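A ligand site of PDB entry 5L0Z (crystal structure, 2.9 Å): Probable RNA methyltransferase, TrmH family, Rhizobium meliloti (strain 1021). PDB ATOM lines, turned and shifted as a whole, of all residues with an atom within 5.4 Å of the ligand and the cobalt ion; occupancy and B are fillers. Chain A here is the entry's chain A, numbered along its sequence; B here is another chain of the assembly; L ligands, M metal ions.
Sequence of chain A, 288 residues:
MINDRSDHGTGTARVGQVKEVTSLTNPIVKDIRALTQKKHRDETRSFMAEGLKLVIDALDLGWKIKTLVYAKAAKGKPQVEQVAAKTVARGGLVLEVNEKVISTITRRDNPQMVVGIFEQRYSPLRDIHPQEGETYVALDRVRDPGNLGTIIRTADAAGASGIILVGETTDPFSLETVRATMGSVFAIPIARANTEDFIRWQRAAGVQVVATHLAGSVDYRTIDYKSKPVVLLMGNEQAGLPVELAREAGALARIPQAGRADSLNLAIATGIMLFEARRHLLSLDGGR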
ATOM      1  N   THR A 212      19.863 -12.921  32.302  1.00  0.00           N
ATOM      2  CA  THR A 212      18.497 -13.369  32.394  1.00  0.00           C
ATOM      3  C   THR A 212      18.231 -14.425  31.348  1.00  0.00           C
ATOM      4  O   THR A 212      18.632 -14.298  30.204  1.00  0.00           O
ATOM      5  CB  THR A 212      17.538 -12.195  32.271  1.00  0.00           C
ATOM      6  OG1 THR A 212      17.760 -11.548  31.019  1.00  0.00           O
ATOM      7  CG2 THR A 212      17.806 -11.192  33.404  1.00  0.00           C
ATOM      8  N   HIS A 213      17.594 -15.509  31.782  1.00  0.00           N
ATOM      9  CA  HIS A 213      17.224 -16.602  30.906  1.00  0.00           C
ATOM     10  C   HIS A 213      15.851 -17.118  31.333  1.00  0.00           C
ATOM     11  O   HIS A 213      15.486 -17.072  32.500  1.00  0.00           O
ATOM     12  CB  HIS A 213      18.263 -17.730  30.984  1.00  0.00           C
ATOM     13  CG  HIS A 213      18.476 -18.449  29.685  1.00  0.00           C
ATOM     14  ND1 HIS A 213      17.441 -18.861  28.870  1.00  0.00           N
ATOM     15  CD2 HIS A 213      19.621 -18.813  29.056  1.00  0.00           C
ATOM     16  CE1 HIS A 213      17.930 -19.449  27.794  1.00  0.00           C
ATOM     17  NE2 HIS A 213      19.256 -19.430  27.884  1.00  0.00           N
ATOM     18  N   LEU A 214      15.071 -17.594  30.377  1.00  0.00           N
ATOM     19  CA  LEU A 214      13.871 -18.336  30.712  1.00  0.00           C
ATOM     20  C   LEU A 214      14.128 -19.707  31.350  1.00  0.00           C
ATOM     21  O   LEU A 214      13.207 -20.272  31.954  1.00  0.00           O
ATOM     22  CB  LEU A 214      12.949 -18.428  29.499  1.00  0.00           C
ATOM     23  CG  LEU A 214      12.426 -17.000  29.273  1.00  0.00           C
ATOM     24  CD1 LEU A 214      12.612 -16.554  27.837  1.00  0.00           C
ATOM     25  CD2 LEU A 214      10.985 -16.883  29.743  1.00  0.00           C
ATOM     26  N   LEU A 233      22.237  -8.273  32.042  1.00  0.00           N
ATOM     27  CA  LEU A 233      22.359  -8.839  30.685  1.00  0.00           C
ATOM     28  C   LEU A 233      21.009  -9.401  30.181  1.00  0.00           C
ATOM     29  O   LEU A 233      20.497 -10.382  30.690  1.00  0.00           O
ATOM     30  CB  LEU A 233      23.458  -9.908  30.658  1.00  0.00           C
ATOM     31  CG  LEU A 233      24.157 -10.140  29.321  1.00  0.00           C
ATOM     32  CD1 LEU A 233      24.857  -8.887  28.831  1.00  0.00           C
ATOM     33  CD2 LEU A 233      25.178 -11.260  29.460  1.00  0.00           C
ATOM     34  N   MET A 234      20.472  -8.742  29.170  1.00  0.00           N
ATOM     35  CA  MET A 234      19.203  -9.106  28.580  1.00  0.00           C
ATOM     36  C   MET A 234      19.481  -9.809  27.278  1.00  0.00           C
ATOM     37  O   MET A 234      20.379  -9.450  26.539  1.00  0.00           O
ATOM     38  CB  MET A 234      18.330  -7.868  28.364  1.00  0.00           C
ATOM     39  CG  MET A 234      18.389  -6.889  29.527  1.00  0.00           C
ATOM     40  SD  MET A 234      17.837  -7.600  31.280  1.00  0.00           S
ATOM     41  CE  MET A 234      16.037  -8.241  30.791  1.00  0.00           C
ATOM     42  N   GLY A 235      18.681 -10.812  26.965  1.00  0.00           N
ATOM     43  CA  GLY A 235      18.798 -11.528  25.704  1.00  0.00           C
ATOM     44  C   GLY A 235      17.990 -11.015  24.514  1.00  0.00           C
ATOM     45  O   GLY A 235      17.052 -10.244  24.649  1.00  0.00           O
ATOM     46  N   ASN A 236      18.390 -11.466  23.333  1.00  0.00           N
ATOM     47  CA  ASN A 236      17.752 -11.188  22.036  1.00  0.00           C
ATOM     48  C   ASN A 236      16.275 -11.544  22.092  1.00  0.00           C
ATOM     49  O   ASN A 236      15.889 -12.449  22.805  1.00  0.00           O
ATOM     50  CB  ASN A 236      18.457 -12.070  20.992  1.00  0.00           C
ATOM     51  CG  ASN A 236      17.842 -11.966  19.642  1.00  0.00           C
ATOM     52  OD1 ASN A 236      17.053 -12.821  19.246  1.00  0.00           O
ATOM     53  ND2 ASN A 236      18.192 -10.902  18.918  1.00  0.00           N
ATOM     54  N   GLU A 237      15.447 -10.852  21.313  1.00  0.00           N
ATOM     55  CA  GLU A 237      13.992 -11.096  21.349  1.00  0.00           C
ATOM     56  C   GLU A 237      13.568 -12.492  20.856  1.00  0.00           C
ATOM     57  O   GLU A 237      12.803 -13.173  21.530  1.00  0.00           O
ATOM     58  CB  GLU A 237      13.203 -10.040  20.560  1.00  0.00           C
ATOM     59  CG  GLU A 237      13.273  -8.623  21.110  1.00  0.00           C
ATOM     60  CD  GLU A 237      14.353  -7.809  20.475  1.00  0.00           C
ATOM     61  OE1 GLU A 237      15.475  -8.358  20.336  1.00  0.00           O
ATOM     62  OE2 GLU A 237      14.099  -6.638  20.102  1.00  0.00           O
ATOM     63  N   GLN A 238      14.044 -12.927  19.699  1.00  0.00           N
ATOM     64  CA  GLN A 238      13.706 -14.267  19.167  1.00  0.00           C
ATOM     65  C   GLN A 238      14.438 -15.396  19.937  1.00  0.00           C
ATOM     66  O   GLN A 238      13.849 -16.431  20.247  1.00  0.00           O
ATOM     67  CB  GLN A 238      13.927 -14.330  17.637  1.00  0.00           C
ATOM     68  CG  GLN A 238      15.371 -14.609  17.152  1.00  0.00           C
ATOM     69  CD  GLN A 238      15.872 -13.673  16.029  1.00  0.00           C
ATOM     70  OE1 GLN A 238      16.695 -12.756  16.254  1.00  0.00           O
ATOM     71  NE2 GLN A 238      15.382 -13.909  14.806  1.00  0.00           N
ATOM     72  N   ALA A 239      15.692 -15.152  20.316  1.00  0.00           N
ATOM     73  CA  ALA A 239      16.635 -16.205  20.671  1.00  0.00           C
ATOM     74  C   ALA A 239      17.040 -16.282  22.129  1.00  0.00           C
ATOM     75  O   ALA A 239      17.376 -17.363  22.602  1.00  0.00           O
ATOM     76  CB  ALA A 239      17.880 -16.018  19.825  1.00  0.00           C
ATOM     77  N   GLY A 240      17.053 -15.183  22.858  1.00  0.00           N
ATOM     78  CA  GLY A 240      17.563 -15.212  24.237  1.00  0.00           C
ATOM     79  C   GLY A 240      19.086 -15.177  24.258  1.00  0.00           C
ATOM     80  O   GLY A 240      19.698 -14.974  23.230  1.00  0.00           O
ATOM     81  N   LEU A 241      19.696 -15.341  25.426  1.00  0.00           N
ATOM     82  CA  LEU A 241      21.152 -15.176  25.515  1.00  0.00           C
ATOM     83  C   LEU A 241      21.905 -16.381  24.958  1.00  0.00           C
ATOM     84  O   LEU A 241      21.526 -17.507  25.234  1.00  0.00           O
ATOM     85  CB  LEU A 241      21.582 -14.911  26.953  1.00  0.00           C
ATOM     86  CG  LEU A 241      21.397 -13.504  27.506  1.00  0.00           C
ATOM     87  CD1 LEU A 241      21.841 -13.517  28.950  1.00  0.00           C
ATOM     88  CD2 LEU A 241      22.150 -12.439  26.728  1.00  0.00           C
ATOM     89  N   ALA A 253      19.359 -15.153  36.355  1.00  0.00           N
ATOM     90  CA  ALA A 253      18.054 -14.824  36.954  1.00  0.00           C
ATOM     91  C   ALA A 253      16.887 -15.014  36.025  1.00  0.00           C
ATOM     92  O   ALA A 253      17.039 -14.991  34.808  1.00  0.00           O
ATOM     93  CB  ALA A 253      18.023 -13.401  37.431  1.00  0.00           C
ATOM     94  N   ARG A 254      15.732 -15.231  36.636  1.00  0.00           N
ATOM     95  CA  ARG A 254      14.479 -15.250  35.900  1.00  0.00           C
ATOM     96  C   ARG A 254      13.309 -14.723  36.735  1.00  0.00           C
ATOM     97  O   ARG A 254      13.245 -14.892  37.964  1.00  0.00           O
ATOM     98  CB  ARG A 254      14.172 -16.634  35.292  1.00  0.00           C
ATOM     99  CG  ARG A 254      13.519 -17.680  36.183  1.00  0.00           C
ATOM    100  CD  ARG A 254      12.915 -18.793  35.338  1.00  0.00           C
ATOM    101  NE  ARG A 254      11.556 -18.427  34.948  1.00  0.00           N
ATOM    102  CZ  ARG A 254      10.455 -19.185  35.121  1.00  0.00           C
ATOM    103  NH1 ARG A 254      10.542 -20.420  35.665  1.00  0.00           N
ATOM    104  NH2 ARG A 254       9.255 -18.719  34.732  1.00  0.00           N
ATOM    105  N   ILE A 255      12.418 -14.023  36.019  1.00  0.00           N
ATOM    106  CA  ILE A 255      11.186 -13.472  36.567  1.00  0.00           C
ATOM    107  C   ILE A 255      10.114 -14.553  36.488  1.00  0.00           C
ATOM    108  O   ILE A 255       9.888 -15.127  35.407  1.00  0.00           O
ATOM    109  CB  ILE A 255      10.749 -12.218  35.782  1.00  0.00           C
ATOM    110  CG1 ILE A 255      11.806 -11.120  35.936  1.00  0.00           C
ATOM    111  CG2 ILE A 255       9.400 -11.693  36.232  1.00  0.00           C
ATOM    112  CD1 ILE A 255      11.783 -10.180  34.762  1.00  0.00           C
ATOM    113  N   PRO A 256       9.497 -14.867  37.643  1.00  0.00           N
ATOM    114  CA  PRO A 256       8.449 -15.893  37.587  1.00  0.00           C
ATOM    115  C   PRO A 256       7.221 -15.450  36.782  1.00  0.00           C
ATOM    116  O   PRO A 256       6.749 -14.321  36.951  1.00  0.00           O
ATOM    117  CB  PRO A 256       8.091 -16.145  39.052  1.00  0.00           C
ATOM    118  CG  PRO A 256       8.673 -14.994  39.808  1.00  0.00           C
ATOM    119  CD  PRO A 256       9.861 -14.528  39.026  1.00  0.00           C
ATOM    120  N   GLN A 257       6.755 -16.325  35.884  1.00  0.00           N
ATOM    121  CA  GLN A 257       5.510 -16.156  35.152  1.00  0.00           C
ATOM    122  C   GLN A 257       4.525 -17.284  35.508  1.00  0.00           C
ATOM    123  O   GLN A 257       4.889 -18.286  36.133  1.00  0.00           O
ATOM    124  CB  GLN A 257       5.760 -16.198  33.672  1.00  0.00           C
ATOM    125  CG  GLN A 257       6.924 -15.370  33.165  1.00  0.00           C
ATOM    126  CD  GLN A 257       7.060 -15.457  31.661  1.00  0.00           C
ATOM    127  OE1 GLN A 257       6.223 -16.035  30.967  1.00  0.00           O
ATOM    128  NE2 GLN A 257       8.099 -14.908  31.146  1.00  0.00           N
ATOM    129  N   ASP A 262       4.823 -17.650  26.925  1.00  0.00           N
ATOM    130  CA  ASP A 262       6.184 -18.107  26.763  1.00  0.00           C
ATOM    131  C   ASP A 262       7.102 -17.232  27.627  1.00  0.00           C
ATOM    132  O   ASP A 262       7.737 -17.702  28.567  1.00  0.00           O
ATOM    133  CB  ASP A 262       6.541 -18.025  25.246  1.00  0.00           C
ATOM    134  CG  ASP A 262       8.035 -18.295  24.939  1.00  0.00           C
ATOM    135  OD1 ASP A 262       8.849 -18.654  25.836  1.00  0.00           O
ATOM    136  OD2 ASP A 262       8.395 -18.121  23.745  1.00  0.00           O
ATOM    137  N   SER A 263       7.130 -15.946  27.298  1.00  0.00           N
ATOM    138  CA  SER A 263       8.107 -15.024  27.842  1.00  0.00           C
ATOM    139  C   SER A 263       7.536 -13.639  27.931  1.00  0.00           C
ATOM    140  O   SER A 263       6.473 -13.362  27.343  1.00  0.00           O
ATOM    141  CB  SER A 263       9.323 -14.971  26.942  1.00  0.00           C
ATOM    142  OG  SER A 263       9.140 -13.925  26.004  1.00  0.00           O
ATOM    143  N   LEU A 264       8.256 -12.771  28.644  1.00  0.00           N
ATOM    144  CA  LEU A 264       7.961 -11.352  28.677  1.00  0.00           C
ATOM    145  C   LEU A 264       8.597 -10.656  27.499  1.00  0.00           C
ATOM    146  O   LEU A 264       9.587 -11.088  26.944  1.00  0.00           O
ATOM    147  CB  LEU A 264       8.481 -10.699  29.934  1.00  0.00           C
ATOM    148  CG  LEU A 264       7.827 -11.156  31.227  1.00  0.00           C
ATOM    149  CD1 LEU A 264       8.817 -10.950  32.341  1.00  0.00           C
ATOM    150  CD2 LEU A 264       6.546 -10.394  31.506  1.00  0.00           C
ATOM    151  N   ASN A 265       7.994  -9.547  27.110  1.00  0.00           N
ATOM    152  CA  ASN A 265       8.567  -8.681  26.100  1.00  0.00           C
ATOM    153  C   ASN A 265       9.886  -8.207  26.659  1.00  0.00           C
ATOM    154  O   ASN A 265      10.027  -8.128  27.877  1.00  0.00           O
ATOM    155  CB  ASN A 265       7.659  -7.489  25.858  1.00  0.00           C
ATOM    156  CG  ASN A 265       8.398  -6.312  25.311  1.00  0.00           C
ATOM    157  OD1 ASN A 265       8.778  -5.427  26.054  1.00  0.00           O
ATOM    158  ND2 ASN A 265       8.673  -6.313  24.029  1.00  0.00           N
ATOM    159  N   LEU A 266      10.843  -7.899  25.788  1.00  0.00           N
ATOM    160  CA  LEU A 266      12.190  -7.545  26.210  1.00  0.00           C
ATOM    161  C   LEU A 266      12.226  -6.314  27.079  1.00  0.00           C
ATOM    162  O   LEU A 266      12.790  -6.323  28.164  1.00  0.00           O
ATOM    163  CB  LEU A 266      13.018  -7.273  24.977  1.00  0.00           C
ATOM    164  CG  LEU A 266      14.438  -6.794  25.215  1.00  0.00           C
ATOM    165  CD1 LEU A 266      15.094  -7.839  26.073  1.00  0.00           C
ATOM    166  CD2 LEU A 266      15.199  -6.579  23.908  1.00  0.00           C
ATOM    167  N   ALA A 269      10.610  -6.894  30.570  1.00  0.00           N
ATOM    168  CA  ALA A 269      11.586  -7.587  31.389  1.00  0.00           C
ATOM    169  C   ALA A 269      12.670  -6.621  31.878  1.00  0.00           C
ATOM    170  O   ALA A 269      12.988  -6.596  33.047  1.00  0.00           O
ATOM    171  CB  ALA A 269      12.201  -8.700  30.586  1.00  0.00           C
ATOM    172  N   ARG B 153      -0.205  -9.025  26.939  1.00  0.00           N
ATOM    173  CA  ARG B 153       0.818 -10.062  27.087  1.00  0.00           C
ATOM    174  C   ARG B 153       1.361 -10.201  28.488  1.00  0.00           C
ATOM    175  O   ARG B 153       1.551 -11.302  28.995  1.00  0.00           O
ATOM    176  CB  ARG B 153       1.975  -9.733  26.183  1.00  0.00           C
ATOM    177  CG  ARG B 153       2.942 -10.847  26.023  1.00  0.00           C
ATOM    178  CD  ARG B 153       3.874 -10.479  24.890  1.00  0.00           C
ATOM    179  NE  ARG B 153       5.101 -11.276  24.936  1.00  0.00           N
ATOM    180  CZ  ARG B 153       6.228 -10.970  24.302  1.00  0.00           C
ATOM    181  NH1 ARG B 153       6.327  -9.866  23.527  1.00  0.00           N
ATOM    182  NH2 ARG B 153       7.282 -11.799  24.423  1.00  0.00           N
HETATM  183  N1  LIG L   1      14.179 -16.947  23.454  1.00  0.00           N
HETATM  184  C1  LIG L   1      13.183 -16.902  24.491  1.00  0.00           C
HETATM  185  C2  LIG L   1      12.306 -18.132  24.337  1.00  0.00           C
HETATM  186  O1  LIG L   1      11.399 -18.154  23.478  1.00  0.00           O
HETATM  187  O2  LIG L   1      12.531 -19.137  25.047  1.00  0.00           O
HETATM  188  C3  LIG L   1      12.399 -15.577  24.410  1.00  0.00           C
HETATM  189  C4  LIG L   1      13.287 -14.329  24.607  1.00  0.00           C
HETATM  190  S1  LIG L   1      12.483 -12.937  25.154  1.00  0.00           S
HETATM  191  C5  LIG L   1      11.237 -12.470  24.136  1.00  0.00           C
HETATM  192  C6  LIG L   1      13.527 -11.649  25.259  1.00  0.00           C
HETATM  193  C7  LIG L   1      14.334 -11.491  26.550  1.00  0.00           C
HETATM  194  O3  LIG L   1      13.531 -10.890  27.577  1.00  0.00           O
HETATM  195  C8  LIG L   1      14.950 -12.726  27.203  1.00  0.00           C
HETATM  196  O4  LIG L   1      16.196 -13.134  26.617  1.00  0.00           O
HETATM  197  C9  LIG L   1      15.156 -12.230  28.602  1.00  0.00           C
HETATM  198  O5  LIG L   1      16.337 -11.438  28.703  1.00  0.00           O
HETATM  199  C10 LIG L   1      13.952 -11.354  28.862  1.00  0.00           C
HETATM  200  N2  LIG L   1      12.871 -12.114  29.553  1.00  0.00           N
HETATM  201  C11 LIG L   1      11.635 -12.399  29.127  1.00  0.00           C
HETATM  202  N3  LIG L   1      10.943 -13.096  30.061  1.00  0.00           N
HETATM  203  C12 LIG L   1      11.741 -13.272  31.116  1.00  0.00           C
HETATM  204  C13 LIG L   1      11.681 -13.911  32.448  1.00  0.00           C
HETATM  205  N4  LIG L   1      10.589 -14.551  32.919  1.00  0.00           N
HETATM  206  N5  LIG L   1      12.782 -13.830  33.224  1.00  0.00           N
HETATM  207  C14 LIG L   1      13.904 -13.205  32.839  1.00  0.00           C
HETATM  208  N6  LIG L   1      14.022 -12.612  31.642  1.00  0.00           N
HETATM  209  C15 LIG L   1      13.008 -12.616  30.766  1.00  0.00           C
HETATM  210 CO    CO M   1      13.634 -19.946  23.399  1.00  0.00          CO
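OD1 of Asn 236 sits at hydrogen-bond distance from N of Ala 239. O of Leu 264 lies within hydrogen-bond range of NH2 of Arg 153 of chain B (3.5 Å). The backbone NH (N) of Leu 264 lies close to the side-chain amide nitrogen (NE2) of Gln 257. The side-chain amide oxygen (OE1) of Gln 238 sits close to the side-chain amide oxygen (OD1) of Asn 236, at 3.0 Å. The side-chain hydroxyl of Thr 212 lies within hydrogen-bond range of the backbone carbonyl oxygen of Leu 233 (3.0 Å). The guanidinium group (NH2) of Arg 153 of chain B sits at hydrogen-bond distance from the side-chain hydroxyl (OG) of Ser 263 (3.2 Å). O of Asp 262 sits close to OE1 of Gln 257, 3.3 Å away.
The backbone carbonyl oxygen of Glu 237 sits close to a sulfur (S1) of the ligand, at 3.6 Å. The side-chain hydroxyl (OG) of Ser 263 lies close to a sulfur (S1) of the ligand (3.6 Å). Leu 214 touches the ligand. CA of Met 234 touches O5 of the ligand (3.7 Å). Asn 236 touches the ligand (O to C6, 3.5 Å). Arg 254 touches the ligand (CA to N5, 3.5 Å). CD1 of Leu 266 touches O3 of the ligand, 3.7 Å away. Ala 269 touches the ligand (CB to C10, 3.6 Å). Hydrophobic or aromatic side chains that line the ligand: Leu 214, Met 234, Ile 255, Leu 264, Leu 266 and Ala 269. 17 residues have an atom within 4 Å of the ligand: Thr 212, Leu 214, Met 234, Gly 235, Asn 236, Glu 237, Gln 238, Ala 239, Gly 240, Arg 254, Ile 255, Gln 257, Asp 262, Ser 263, Leu 264, Leu 266 and Ala 269. The nearest printed residue that does not touch the ligand is Arg 153 of chain B (4.02 Å).
OD2 of Asp 262 sits close to O1 of the ligand, at 3.0 Å. NE2 of Gln 257 lies close to N4 of the ligand. N of Ile 255 is in hydrogen-bond range of N5 of the ligand, 2.8 Å away. N of Gly 235 lies within hydrogen-bond range of O5 of the ligand, 3.0 Å away. The backbone NH of Gly 240 sits close to a nitrogen (N1) of the ligand (3.4 Å). The backbone carbonyl oxygen (O) of Ile 255 lies within hydrogen-bond range of a nitrogen (N4) of the ligand (2.6 Å). N1 of the ligand lies within hydrogen-bond range of O of Gln 238, at 3.3 Å. The side-chain hydroxyl (OG1) of Thr 212 lies within hydrogen-bond range of an oxygen (O5) of the ligand (2.7 Å). A nitrogen (N3) of the ligand sits at hydrogen-bond distance from the backbone NH (N) of Leu 264. O of Ala 239 lies close to N1 of the ligand (3.3 Å).
The cobalt ion is bound by an oxygen (O2) of the ligand, at 2.1 Å.
No residue comes within 4 Å of the cobalt ion.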
